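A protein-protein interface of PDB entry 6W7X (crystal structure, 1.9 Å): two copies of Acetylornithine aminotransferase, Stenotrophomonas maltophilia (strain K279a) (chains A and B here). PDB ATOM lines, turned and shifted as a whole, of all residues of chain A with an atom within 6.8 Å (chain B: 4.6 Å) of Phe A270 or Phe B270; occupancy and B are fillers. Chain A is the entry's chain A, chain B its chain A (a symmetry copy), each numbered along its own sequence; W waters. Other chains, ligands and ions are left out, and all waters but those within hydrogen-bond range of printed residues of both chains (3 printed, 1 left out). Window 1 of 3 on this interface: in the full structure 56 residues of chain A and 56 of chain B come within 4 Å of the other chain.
Of the printed residues of chain B, Leu A69 touches Trp B81. Of the printed residues of chain B, Trp A81 touches Leu B73 (3.7 Å), Gly B269 (3.99 Å), Phe B270 (3.8 Å) and Val B303 (3.8 Å). Of chain B, only Trp B81, Phe B270 and Leu B299 come within 4 Å of Phe A270. Printed residues of chain B within 4 Å of Leu A299: Leu B73 and Phe B270. Printed residues of chain A within 4 Å of Trp B81: Leu A69, Leu A73, Gly A269, Phe A270 and Val A303. Of chain A, only Trp A81 (3.8 Å), Phe A270 (3.4 Å) and Leu A299 (3.8 Å) come within 4 Å of Phe B270. Printed residues of chain A within 4 Å of Val B303: Trp A81 (3.8 Å). The nearest residue of chain B that does not touch Phe A270 is Pro B271 (4.3 Å). The nearest residue of chain A that does not touch Phe B270 is Pro A271 (4.3 Å).
NZ of Lys B264 sits at hydrogen-bond distance from ND1 of His A82 (3.1 Å).
O of Ile B272 is in hydrogen-bond range of N of Lys B264 (3.1 Å). The side-chain amide oxygen (OD1) of Asn A297 lies within hydrogen-bond range of the backbone NH (N) of Ala A300 (2.8 Å). N of Ile A272 sits at hydrogen-bond distance from O of Asn A113, 3.4 Å away. The side-chain amide oxygen (OD1) of Asn A297 is in hydrogen-bond range of the backbone NH (N) of Leu A299 (3.1 Å). The backbone NH (N) of Gly A269 is in hydrogen-bond range of the backbone carbonyl oxygen (O) of Lys A264 (3.0 Å). The backbone NH (N) of Gly B269 sits at hydrogen-bond distance from the backbone carbonyl oxygen (O) of Lys B264, at 3.0 Å.
Leu A73 touches Trp B81, and with the chains exchanged Trp A81 touches Leu B73. Trp A81 touches Gly B269, and with the chains exchanged Gly A269 touches Trp B81. Trp A81 touches Phe B270, and with the chains exchanged Phe A270 touches Trp B81. Phe A270 touches Leu B299, and with the chains exchanged Leu A299 touches Phe B270. Positions printed for both chains: 73, 81, 264, 267, 268, 269, 270, 271, 272, 299, 300 and 303. Of the 19 pairs that touch across the chains among the printed residues, 13 have their exchanged pair printed and touching as well.
Of the 23 printed residues of chain A, 10 touch a printed residue of chain B. Printed residues of chain A that touch a printed residue of chain B: Leu A69, Leu A73, Trp A81, His A82, Asn A113, Gly A269, Phe A270, Asn A297, Leu A299 and Val A303. Hydrophobic or aromatic side chains of chain B within 4 Å of the printed part of chain A: Leu B73, Trp B81, Phe B270, Pro B271, Leu B299 and Val B303.
Water W2 lies within hydrogen-bond range of the side-chain amino group (NZ) of Lys B264 (2.6 Å) and the side-chain amide oxygen (OD1) of Asn A113 (2.6 Å). Water W1 lies within hydrogen-bond range of the backbone carbonyl oxygen of Gly A269 (2.7 Å), the side-chain amino group of Lys A264 (2.8 Å) and the backbone carbonyl oxygen of Trp B81 (2.9 Å). Water W3 bridges NZ of Lys B264 (2.9 Å) and ND1 of His A82 (3.5 Å).
Trp A81 touches Leu B73. CE3 of Trp A81 touches C of Gly B269 (3.99 Å). CZ3 of Trp A81 touches CG1 of Val B303, 3.8 Å away. His A82 touches Gly B269 (CB to O, 3.8 Å). Asn A113 touches Pro B271. N of Phe A270 touches CE3 of Trp B81 (3.8 Å). Lys B264 touches Asn A297. Pro B271 touches Asn A297 (CG to ND2, 3.8 Å). Leu B73 touches Leu A299 (CD2 to CD2, 3.9 Å). Leu A299 touches Phe B270 (CD2 to CD1, 3.8 Å).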
ATOM      1  N   VAL A  59      -7.905 -26.469 -29.228  1.00  0.00           N
ATOM      2  CA  VAL A  59      -9.272 -26.952 -29.339  1.00  0.00           C
ATOM      3  C   VAL A  59      -9.596 -27.380 -30.764  1.00  0.00           C
ATOM      4  O   VAL A  59     -10.115 -28.476 -30.988  1.00  0.00           O
ATOM      5  CB  VAL A  59     -10.275 -25.888 -28.838  1.00  0.00           C
ATOM      6  CG1 VAL A  59     -11.670 -26.204 -29.327  1.00  0.00           C
ATOM      7  CG2 VAL A  59     -10.240 -25.806 -27.323  1.00  0.00           C
ATOM      8  N   LEU A  69     -16.027 -32.086 -40.592  1.00  0.00           N
ATOM      9  CA  LEU A  69     -16.681 -31.606 -39.375  1.00  0.00           C
ATOM     10  C   LEU A  69     -17.945 -30.820 -39.699  1.00  0.00           C
ATOM     11  O   LEU A  69     -18.992 -31.022 -39.073  1.00  0.00           O
ATOM     12  CB  LEU A  69     -15.722 -30.745 -38.555  1.00  0.00           C
ATOM     13  CG  LEU A  69     -14.542 -31.465 -37.896  1.00  0.00           C
ATOM     14  CD1 LEU A  69     -13.864 -30.531 -36.911  1.00  0.00           C
ATOM     15  CD2 LEU A  69     -15.020 -32.739 -37.207  1.00  0.00           C
ATOM     16  N   LEU A  73     -21.909 -31.705 -38.853  1.00  0.00           N
ATOM     17  CA  LEU A  73     -22.758 -30.809 -38.076  1.00  0.00           C
ATOM     18  C   LEU A  73     -24.022 -30.461 -38.853  1.00  0.00           C
ATOM     19  O   LEU A  73     -25.134 -30.544 -38.323  1.00  0.00           O
ATOM     20  CB  LEU A  73     -21.988 -29.547 -37.691  1.00  0.00           C
ATOM     21  CG  LEU A  73     -22.891 -28.510 -37.004  1.00  0.00           C
ATOM     22  CD1 LEU A  73     -23.537 -29.117 -35.778  1.00  0.00           C
ATOM     23  CD2 LEU A  73     -22.129 -27.252 -36.622  1.00  0.00           C
ATOM     24  N   TRP A  81     -31.507 -32.168 -32.325  1.00  0.00           N
ATOM     25  CA  TRP A  81     -30.406 -31.568 -31.587  1.00  0.00           C
ATOM     26  C   TRP A  81     -30.243 -32.111 -30.182  1.00  0.00           C
ATOM     27  O   TRP A  81     -29.131 -32.079 -29.648  1.00  0.00           O
ATOM     28  CB  TRP A  81     -30.587 -30.055 -31.482  1.00  0.00           C
ATOM     29  CG  TRP A  81     -30.510 -29.331 -32.777  1.00  0.00           C
ATOM     30  CD1 TRP A  81     -30.456 -29.872 -34.031  1.00  0.00           C
ATOM     31  CD2 TRP A  81     -30.475 -27.914 -32.950  1.00  0.00           C
ATOM     32  NE1 TRP A  81     -30.388 -28.872 -34.973  1.00  0.00           N
ATOM     33  CE2 TRP A  81     -30.402 -27.661 -34.332  1.00  0.00           C
ATOM     34  CE3 TRP A  81     -30.491 -26.831 -32.068  1.00  0.00           C
ATOM     35  CZ2 TRP A  81     -30.346 -26.371 -34.849  1.00  0.00           C
ATOM     36  CZ3 TRP A  81     -30.442 -25.561 -32.583  1.00  0.00           C
ATOM     37  CH2 TRP A  81     -30.364 -25.339 -33.958  1.00  0.00           C
ATOM     38  N   HIS A  82     -31.320 -32.585 -29.562  1.00  0.00           N
ATOM     39  CA  HIS A  82     -31.337 -32.743 -28.116  1.00  0.00           C
ATOM     40  C   HIS A  82     -32.462 -33.696 -27.741  1.00  0.00           C
ATOM     41  O   HIS A  82     -33.553 -33.628 -28.313  1.00  0.00           O
ATOM     42  CB  HIS A  82     -31.525 -31.377 -27.441  1.00  0.00           C
ATOM     43  CG  HIS A  82     -31.894 -31.457 -25.995  1.00  0.00           C
ATOM     44  ND1 HIS A  82     -30.961 -31.651 -24.998  1.00  0.00           N
ATOM     45  CD2 HIS A  82     -33.096 -31.359 -25.377  1.00  0.00           C
ATOM     46  CE1 HIS A  82     -31.572 -31.678 -23.828  1.00  0.00           C
ATOM     47  NE2 HIS A  82     -32.868 -31.494 -24.028  1.00  0.00           N
ATOM     48  N   ASN A 113     -20.809 -31.419 -21.473  1.00  0.00           N
ATOM     49  CA  ASN A 113     -20.803 -30.250 -22.336  1.00  0.00           C
ATOM     50  C   ASN A 113     -19.496 -29.484 -22.328  1.00  0.00           C
ATOM     51  O   ASN A 113     -19.365 -28.532 -23.101  1.00  0.00           O
ATOM     52  CB  ASN A 113     -21.948 -29.312 -21.941  1.00  0.00           C
ATOM     53  CG  ASN A 113     -23.295 -29.957 -22.144  1.00  0.00           C
ATOM     54  OD1 ASN A 113     -23.662 -30.298 -23.269  1.00  0.00           O
ATOM     55  ND2 ASN A 113     -24.024 -30.162 -21.058  1.00  0.00           N
ATOM     56  N   ALA A 263     -12.237 -32.419 -23.265  1.00  0.00           N
ATOM     57  CA  ALA A 263     -13.107 -31.254 -23.416  1.00  0.00           C
ATOM     58  C   ALA A 263     -13.491 -31.101 -24.880  1.00  0.00           C
ATOM     59  O   ALA A 263     -13.626 -32.112 -25.576  1.00  0.00           O
ATOM     60  CB  ALA A 263     -12.433 -29.992 -22.887  1.00  0.00           C
ATOM     61  N   LYS A 264     -13.660 -29.859 -25.364  1.00  0.00           N
ATOM     62  CA  LYS A 264     -14.264 -29.654 -26.679  1.00  0.00           C
ATOM     63  C   LYS A 264     -13.306 -29.921 -27.838  1.00  0.00           C
ATOM     64  O   LYS A 264     -13.752 -29.951 -28.989  1.00  0.00           O
ATOM     65  CB  LYS A 264     -14.882 -28.239 -26.789  1.00  0.00           C
ATOM     66  CG  LYS A 264     -13.939 -27.082 -26.686  1.00  0.00           C
ATOM     67  CD  LYS A 264     -14.715 -25.763 -26.454  1.00  0.00           C
ATOM     68  CE  LYS A 264     -15.675 -25.417 -27.594  1.00  0.00           C
ATOM     69  NZ  LYS A 264     -16.358 -24.064 -27.377  1.00  0.00           N
ATOM     70  N   ALA A 265     -12.021 -30.170 -27.572  1.00  0.00           N
ATOM     71  CA  ALA A 265     -11.184 -30.784 -28.598  1.00  0.00           C
ATOM     72  C   ALA A 265     -11.781 -32.109 -29.087  1.00  0.00           C
ATOM     73  O   ALA A 265     -11.614 -32.478 -30.257  1.00  0.00           O
ATOM     74  CB  ALA A 265      -9.765 -30.992 -28.057  1.00  0.00           C
ATOM     75  N   LEU A 266     -12.487 -32.834 -28.217  1.00  0.00           N
ATOM     76  CA  LEU A 266     -13.196 -34.033 -28.658  1.00  0.00           C
ATOM     77  C   LEU A 266     -14.197 -33.719 -29.767  1.00  0.00           C
ATOM     78  O   LEU A 266     -14.486 -34.575 -30.613  1.00  0.00           O
ATOM     79  CB  LEU A 266     -13.921 -34.672 -27.473  1.00  0.00           C
ATOM     80  CG  LEU A 266     -14.857 -35.859 -27.742  1.00  0.00           C
ATOM     81  CD1 LEU A 266     -14.108 -37.022 -28.441  1.00  0.00           C
ATOM     82  CD2 LEU A 266     -15.506 -36.337 -26.450  1.00  0.00           C
ATOM     83  N   GLY A 267     -14.741 -32.510 -29.773  1.00  0.00           N
ATOM     84  CA  GLY A 267     -15.697 -32.128 -30.795  1.00  0.00           C
ATOM     85  C   GLY A 267     -15.098 -31.275 -31.894  1.00  0.00           C
ATOM     86  O   GLY A 267     -15.836 -30.663 -32.675  1.00  0.00           O
ATOM     87  N   GLY A 268     -13.766 -31.227 -31.963  1.00  0.00           N
ATOM     88  CA  GLY A 268     -13.080 -30.367 -32.914  1.00  0.00           C
ATOM     89  C   GLY A 268     -13.414 -28.900 -32.767  1.00  0.00           C
ATOM     90  O   GLY A 268     -13.184 -28.121 -33.700  1.00  0.00           O
ATOM     91  N   GLY A 269     -13.939 -28.493 -31.611  1.00  0.00           N
ATOM     92  CA  GLY A 269     -14.415 -27.141 -31.399  1.00  0.00           C
ATOM     93  C   GLY A 269     -15.902 -27.039 -31.140  1.00  0.00           C
ATOM     94  O   GLY A 269     -16.379 -25.942 -30.809  1.00  0.00           O
ATOM     95  N   PHE A 270     -16.660 -28.129 -31.311  1.00  0.00           N
ATOM     96  CA  PHE A 270     -18.068 -28.098 -30.912  1.00  0.00           C
ATOM     97  C   PHE A 270     -18.160 -28.347 -29.405  1.00  0.00           C
ATOM     98  O   PHE A 270     -17.412 -29.167 -28.873  1.00  0.00           O
ATOM     99  CB  PHE A 270     -18.867 -29.163 -31.676  1.00  0.00           C
ATOM    100  CG  PHE A 270     -20.365 -29.029 -31.532  1.00  0.00           C
ATOM    101  CD1 PHE A 270     -21.112 -28.382 -32.501  1.00  0.00           C
ATOM    102  CD2 PHE A 270     -21.013 -29.537 -30.420  1.00  0.00           C
ATOM    103  CE1 PHE A 270     -22.491 -28.240 -32.371  1.00  0.00           C
ATOM    104  CE2 PHE A 270     -22.381 -29.400 -30.271  1.00  0.00           C
ATOM    105  CZ  PHE A 270     -23.129 -28.747 -31.252  1.00  0.00           C
ATOM    106  N   PRO A 271     -19.035 -27.643 -28.683  1.00  0.00           N
ATOM    107  CA  PRO A 271     -19.075 -27.807 -27.218  1.00  0.00           C
ATOM    108  C   PRO A 271     -19.374 -29.241 -26.811  1.00  0.00           C
ATOM    109  O   PRO A 271     -20.443 -29.784 -27.101  1.00  0.00           O
ATOM    110  CB  PRO A 271     -20.200 -26.857 -26.788  1.00  0.00           C
ATOM    111  CG  PRO A 271     -20.280 -25.831 -27.874  1.00  0.00           C
ATOM    112  CD  PRO A 271     -19.929 -26.570 -29.149  1.00  0.00           C
ATOM    113  N   ILE A 272     -18.419 -29.854 -26.110  1.00  0.00           N
ATOM    114  CA  ILE A 272     -18.573 -31.219 -25.626  1.00  0.00           C
ATOM    115  C   ILE A 272     -17.495 -31.459 -24.577  1.00  0.00           C
ATOM    116  O   ILE A 272     -16.520 -30.710 -24.483  1.00  0.00           O
ATOM    117  CB  ILE A 272     -18.462 -32.238 -26.792  1.00  0.00           C
ATOM    118  CG1 ILE A 272     -18.924 -33.630 -26.345  1.00  0.00           C
ATOM    119  CG2 ILE A 272     -17.034 -32.302 -27.292  1.00  0.00           C
ATOM    120  CD1 ILE A 272     -19.073 -34.638 -27.495  1.00  0.00           C
ATOM    121  N   GLY A 273     -17.691 -32.488 -23.757  1.00  0.00           N
ATOM    122  CA  GLY A 273     -16.628 -32.992 -22.903  1.00  0.00           C
ATOM    123  C   GLY A 273     -16.961 -34.424 -22.560  1.00  0.00           C
ATOM    124  O   GLY A 273     -18.058 -34.916 -22.841  1.00  0.00           O
ATOM    125  N   ASN A 297     -25.719 -35.360 -26.138  1.00  0.00           N
ATOM    126  CA  ASN A 297     -26.750 -34.931 -27.077  1.00  0.00           C
ATOM    127  C   ASN A 297     -26.321 -35.317 -28.483  1.00  0.00           C
ATOM    128  O   ASN A 297     -25.119 -35.458 -28.750  1.00  0.00           O
ATOM    129  CB  ASN A 297     -27.019 -33.410 -26.990  1.00  0.00           C
ATOM    130  CG  ASN A 297     -25.842 -32.562 -27.469  1.00  0.00           C
ATOM    131  OD1 ASN A 297     -25.716 -32.270 -28.661  1.00  0.00           O
ATOM    132  ND2 ASN A 297     -24.996 -32.147 -26.540  1.00  0.00           N
ATOM    133  N   LEU A 299     -26.271 -33.724 -31.326  1.00  0.00           N
ATOM    134  CA  LEU A 299     -25.575 -32.732 -32.141  1.00  0.00           C
ATOM    135  C   LEU A 299     -24.073 -32.752 -31.870  1.00  0.00           C
ATOM    136  O   LEU A 299     -23.263 -32.847 -32.802  1.00  0.00           O
ATOM    137  CB  LEU A 299     -26.156 -31.343 -31.884  1.00  0.00           C
ATOM    138  CG  LEU A 299     -26.014 -30.301 -33.000  1.00  0.00           C
ATOM    139  CD1 LEU A 299     -26.502 -30.834 -34.341  1.00  0.00           C
ATOM    140  CD2 LEU A 299     -26.764 -29.033 -32.648  1.00  0.00           C
ATOM    141  N   ALA A 300     -23.681 -32.655 -30.598  1.00  0.00           N
ATOM    142  CA  ALA A 300     -22.267 -32.775 -30.257  1.00  0.00           C
ATOM    143  C   ALA A 300     -21.722 -34.138 -30.639  1.00  0.00           C
ATOM    144  O   ALA A 300     -20.575 -34.253 -31.085  1.00  0.00           O
ATOM    145  CB  ALA A 300     -22.054 -32.534 -28.764  1.00  0.00           C
ATOM    146  N   ALA A 301     -22.511 -35.191 -30.439  1.00  0.00           N
ATOM    147  CA  ALA A 301     -21.967 -36.531 -30.631  1.00  0.00           C
ATOM    148  C   ALA A 301     -21.696 -36.803 -32.107  1.00  0.00           C
ATOM    149  O   ALA A 301     -20.644 -37.340 -32.462  1.00  0.00           O
ATOM    150  CB  ALA A 301     -22.911 -37.573 -30.038  1.00  0.00           C
ATOM    151  N   VAL A 303     -20.829 -34.782 -34.390  1.00  0.00           N
ATOM    152  CA  VAL A 303     -19.602 -34.094 -34.774  1.00  0.00           C
ATOM    153  C   VAL A 303     -18.386 -34.764 -34.136  1.00  0.00           C
ATOM    154  O   VAL A 303     -17.367 -34.987 -34.799  1.00  0.00           O
ATOM    155  CB  VAL A 303     -19.685 -32.606 -34.400  1.00  0.00           C
ATOM    156  CG1 VAL A 303     -18.350 -31.929 -34.628  1.00  0.00           C
ATOM    157  CG2 VAL A 303     -20.805 -31.907 -35.189  1.00  0.00           C
ATOM    158  N   ALA A 304     -18.470 -35.096 -32.842  1.00  0.00           N
ATOM    159  CA  ALA A 304     -17.322 -35.701 -32.170  1.00  0.00           C
ATOM    160  C   ALA A 304     -16.943 -37.045 -32.777  1.00  0.00           C
ATOM    161  O   ALA A 304     -15.761 -37.416 -32.759  1.00  0.00           O
ATOM    162  CB  ALA A 304     -17.597 -35.861 -30.673  1.00  0.00           C
ATOM    163  N   LEU B  73     -27.777 -21.890 -37.328  1.00  0.00           N
ATOM    164  CA  LEU B  73     -26.695 -22.816 -37.014  1.00  0.00           C
ATOM    165  C   LEU B  73     -25.861 -23.108 -38.257  1.00  0.00           C
ATOM    166  O   LEU B  73     -24.629 -23.041 -38.223  1.00  0.00           O
ATOM    167  CB  LEU B  73     -27.254 -24.106 -36.416  1.00  0.00           C
ATOM    168  CG  LEU B  73     -26.161 -25.168 -36.213  1.00  0.00           C
ATOM    169  CD1 LEU B  73     -25.065 -24.618 -35.327  1.00  0.00           C
ATOM    170  CD2 LEU B  73     -26.715 -26.453 -35.621  1.00  0.00           C
ATOM    171  N   TRP B  81     -16.345 -21.665 -35.271  1.00  0.00           N
ATOM    172  CA  TRP B  81     -17.056 -22.316 -34.181  1.00  0.00           C
ATOM    173  C   TRP B  81     -16.626 -21.850 -32.805  1.00  0.00           C
ATOM    174  O   TRP B  81     -17.424 -21.922 -31.867  1.00  0.00           O
ATOM    175  CB  TRP B  81     -16.865 -23.830 -34.239  1.00  0.00           C
ATOM    176  CG  TRP B  81     -17.472 -24.485 -35.427  1.00  0.00           C
ATOM    177  CD1 TRP B  81     -18.028 -23.879 -36.519  1.00  0.00           C
ATOM    178  CD2 TRP B  81     -17.591 -25.891 -35.645  1.00  0.00           C
ATOM    179  NE1 TRP B  81     -18.485 -24.829 -37.403  1.00  0.00           N
ATOM    180  CE2 TRP B  81     -18.224 -26.071 -36.888  1.00  0.00           C
ATOM    181  CE3 TRP B  81     -17.228 -27.019 -34.905  1.00  0.00           C
ATOM    182  CZ2 TRP B  81     -18.500 -27.333 -37.405  1.00  0.00           C
ATOM    183  CZ3 TRP B  81     -17.497 -28.261 -35.422  1.00  0.00           C
ATOM    184  CH2 TRP B  81     -18.133 -28.410 -36.655  1.00  0.00           C
ATOM    185  N   LYS B 264     -29.822 -24.541 -21.765  1.00  0.00           N
ATOM    186  CA  LYS B 264     -29.810 -24.669 -23.222  1.00  0.00           C
ATOM    187  C   LYS B 264     -31.154 -24.352 -23.872  1.00  0.00           C
ATOM    188  O   LYS B 264     -31.217 -24.256 -25.102  1.00  0.00           O
ATOM    189  CB  LYS B 264     -29.307 -26.069 -23.649  1.00  0.00           C
ATOM    190  CG  LYS B 264     -30.139 -27.240 -23.231  1.00  0.00           C
ATOM    191  CD  LYS B 264     -29.350 -28.562 -23.406  1.00  0.00           C
ATOM    192  CE  LYS B 264     -28.943 -28.836 -24.855  1.00  0.00           C
ATOM    193  NZ  LYS B 264     -28.247 -30.190 -25.008  1.00  0.00           N
ATOM    194  N   GLY B 267     -30.605 -21.649 -26.084  1.00  0.00           N
ATOM    195  CA  GLY B 267     -30.155 -21.965 -27.426  1.00  0.00           C
ATOM    196  C   GLY B 267     -31.158 -22.765 -28.229  1.00  0.00           C
ATOM    197  O   GLY B 267     -30.811 -23.327 -29.274  1.00  0.00           O
ATOM    198  N   GLY B 268     -32.403 -22.824 -27.751  1.00  0.00           N
ATOM    199  CA  GLY B 268     -33.427 -23.641 -28.383  1.00  0.00           C
ATOM    200  C   GLY B 268     -33.079 -25.110 -28.463  1.00  0.00           C
ATOM    201  O   GLY B 268     -33.678 -25.841 -29.261  1.00  0.00           O
ATOM    202  N   GLY B 269     -32.132 -25.571 -27.646  1.00  0.00           N
ATOM    203  CA  GLY B 269     -31.627 -26.927 -27.718  1.00  0.00           C
ATOM    204  C   GLY B 269     -30.165 -27.026 -28.094  1.00  0.00           C
ATOM    205  O   GLY B 269     -29.607 -28.133 -28.045  1.00  0.00           O
ATOM    206  N   PHE B 270     -29.531 -25.919 -28.501  1.00  0.00           N
ATOM    207  CA  PHE B 270     -28.082 -25.956 -28.714  1.00  0.00           C
ATOM    208  C   PHE B 270     -27.381 -25.786 -27.365  1.00  0.00           C
ATOM    209  O   PHE B 270     -27.837 -25.004 -26.532  1.00  0.00           O
ATOM    210  CB  PHE B 270     -27.653 -24.843 -29.681  1.00  0.00           C
ATOM    211  CG  PHE B 270     -26.228 -24.967 -30.167  1.00  0.00           C
ATOM    212  CD1 PHE B 270     -25.950 -25.553 -31.390  1.00  0.00           C
ATOM    213  CD2 PHE B 270     -25.178 -24.511 -29.392  1.00  0.00           C
ATOM    214  CE1 PHE B 270     -24.639 -25.687 -31.842  1.00  0.00           C
ATOM    215  CE2 PHE B 270     -23.869 -24.642 -29.821  1.00  0.00           C
ATOM    216  CZ  PHE B 270     -23.595 -25.233 -31.055  1.00  0.00           C
ATOM    217  N   PRO B 271     -26.296 -26.517 -27.101  1.00  0.00           N
ATOM    218  CA  PRO B 271     -25.659 -26.431 -25.774  1.00  0.00           C
ATOM    219  C   PRO B 271     -25.205 -25.016 -25.449  1.00  0.00           C
ATOM    220  O   PRO B 271     -24.340 -24.448 -26.121  1.00  0.00           O
ATOM    221  CB  PRO B 271     -24.468 -27.389 -25.892  1.00  0.00           C
ATOM    222  CG  PRO B 271     -24.849 -28.356 -26.968  1.00  0.00           C
ATOM    223  CD  PRO B 271     -25.681 -27.554 -27.948  1.00  0.00           C
ATOM    224  N   ILE B 272     -25.782 -24.452 -24.388  1.00  0.00           N
ATOM    225  CA  ILE B 272     -25.430 -23.113 -23.937  1.00  0.00           C
ATOM    226  C   ILE B 272     -25.982 -22.942 -22.529  1.00  0.00           C
ATOM    227  O   ILE B 272     -26.843 -23.706 -22.085  1.00  0.00           O
ATOM    228  CB  ILE B 272     -25.995 -22.036 -24.901  1.00  0.00           C
ATOM    229  CG1 ILE B 272     -25.375 -20.664 -24.608  1.00  0.00           C
ATOM    230  CG2 ILE B 272     -27.502 -21.961 -24.770  1.00  0.00           C
ATOM    231  CD1 ILE B 272     -25.696 -19.595 -25.664  1.00  0.00           C
ATOM    232  N   LEU B 299     -20.700 -20.224 -32.142  1.00  0.00           N
ATOM    233  CA  LEU B 299     -21.679 -21.179 -32.653  1.00  0.00           C
ATOM    234  C   LEU B 299     -22.940 -21.189 -31.792  1.00  0.00           C
ATOM    235  O   LEU B 299     -24.058 -21.055 -32.305  1.00  0.00           O
ATOM    236  CB  LEU B 299     -21.059 -22.573 -32.729  1.00  0.00           C
ATOM    237  CG  LEU B 299     -21.656 -23.555 -33.743  1.00  0.00           C
ATOM    238  CD1 LEU B 299     -21.753 -22.946 -35.136  1.00  0.00           C
ATOM    239  CD2 LEU B 299     -20.843 -24.832 -33.796  1.00  0.00           C
ATOM    240  N   ALA B 300     -22.780 -21.358 -30.477  1.00  0.00           N
ATOM    241  CA  ALA B 300     -23.929 -21.274 -29.583  1.00  0.00           C
ATOM    242  C   ALA B 300     -24.567 -19.898 -29.637  1.00  0.00           C
ATOM    243  O   ALA B 300     -25.795 -19.773 -29.570  1.00  0.00           O
ATOM    244  CB  ALA B 300     -23.517 -21.595 -28.149  1.00  0.00           C
ATOM    245  N   VAL B 303     -26.906 -19.066 -32.657  1.00  0.00           N
ATOM    246  CA  VAL B 303     -28.190 -19.747 -32.543  1.00  0.00           C
ATOM    247  C   VAL B 303     -29.034 -19.125 -31.430  1.00  0.00           C
ATOM    248  O   VAL B 303     -30.232 -18.878 -31.606  1.00  0.00           O
ATOM    249  CB  VAL B 303     -27.979 -21.252 -32.314  1.00  0.00           C
ATOM    250  CG1 VAL B 303     -29.299 -21.930 -32.013  1.00  0.00           C
ATOM    251  CG2 VAL B 303     -27.286 -21.895 -33.528  1.00  0.00           C
HETATM  252  O   HOH W   1     -17.791 -23.927 -29.791  1.00  0.00           O
HETATM  253  O   HOH W   2     -26.143 -29.795 -23.614  1.00  0.00           O
HETATM  254  O   HOH W   3     -28.206 -32.264 -22.950  1.00  0.00           O
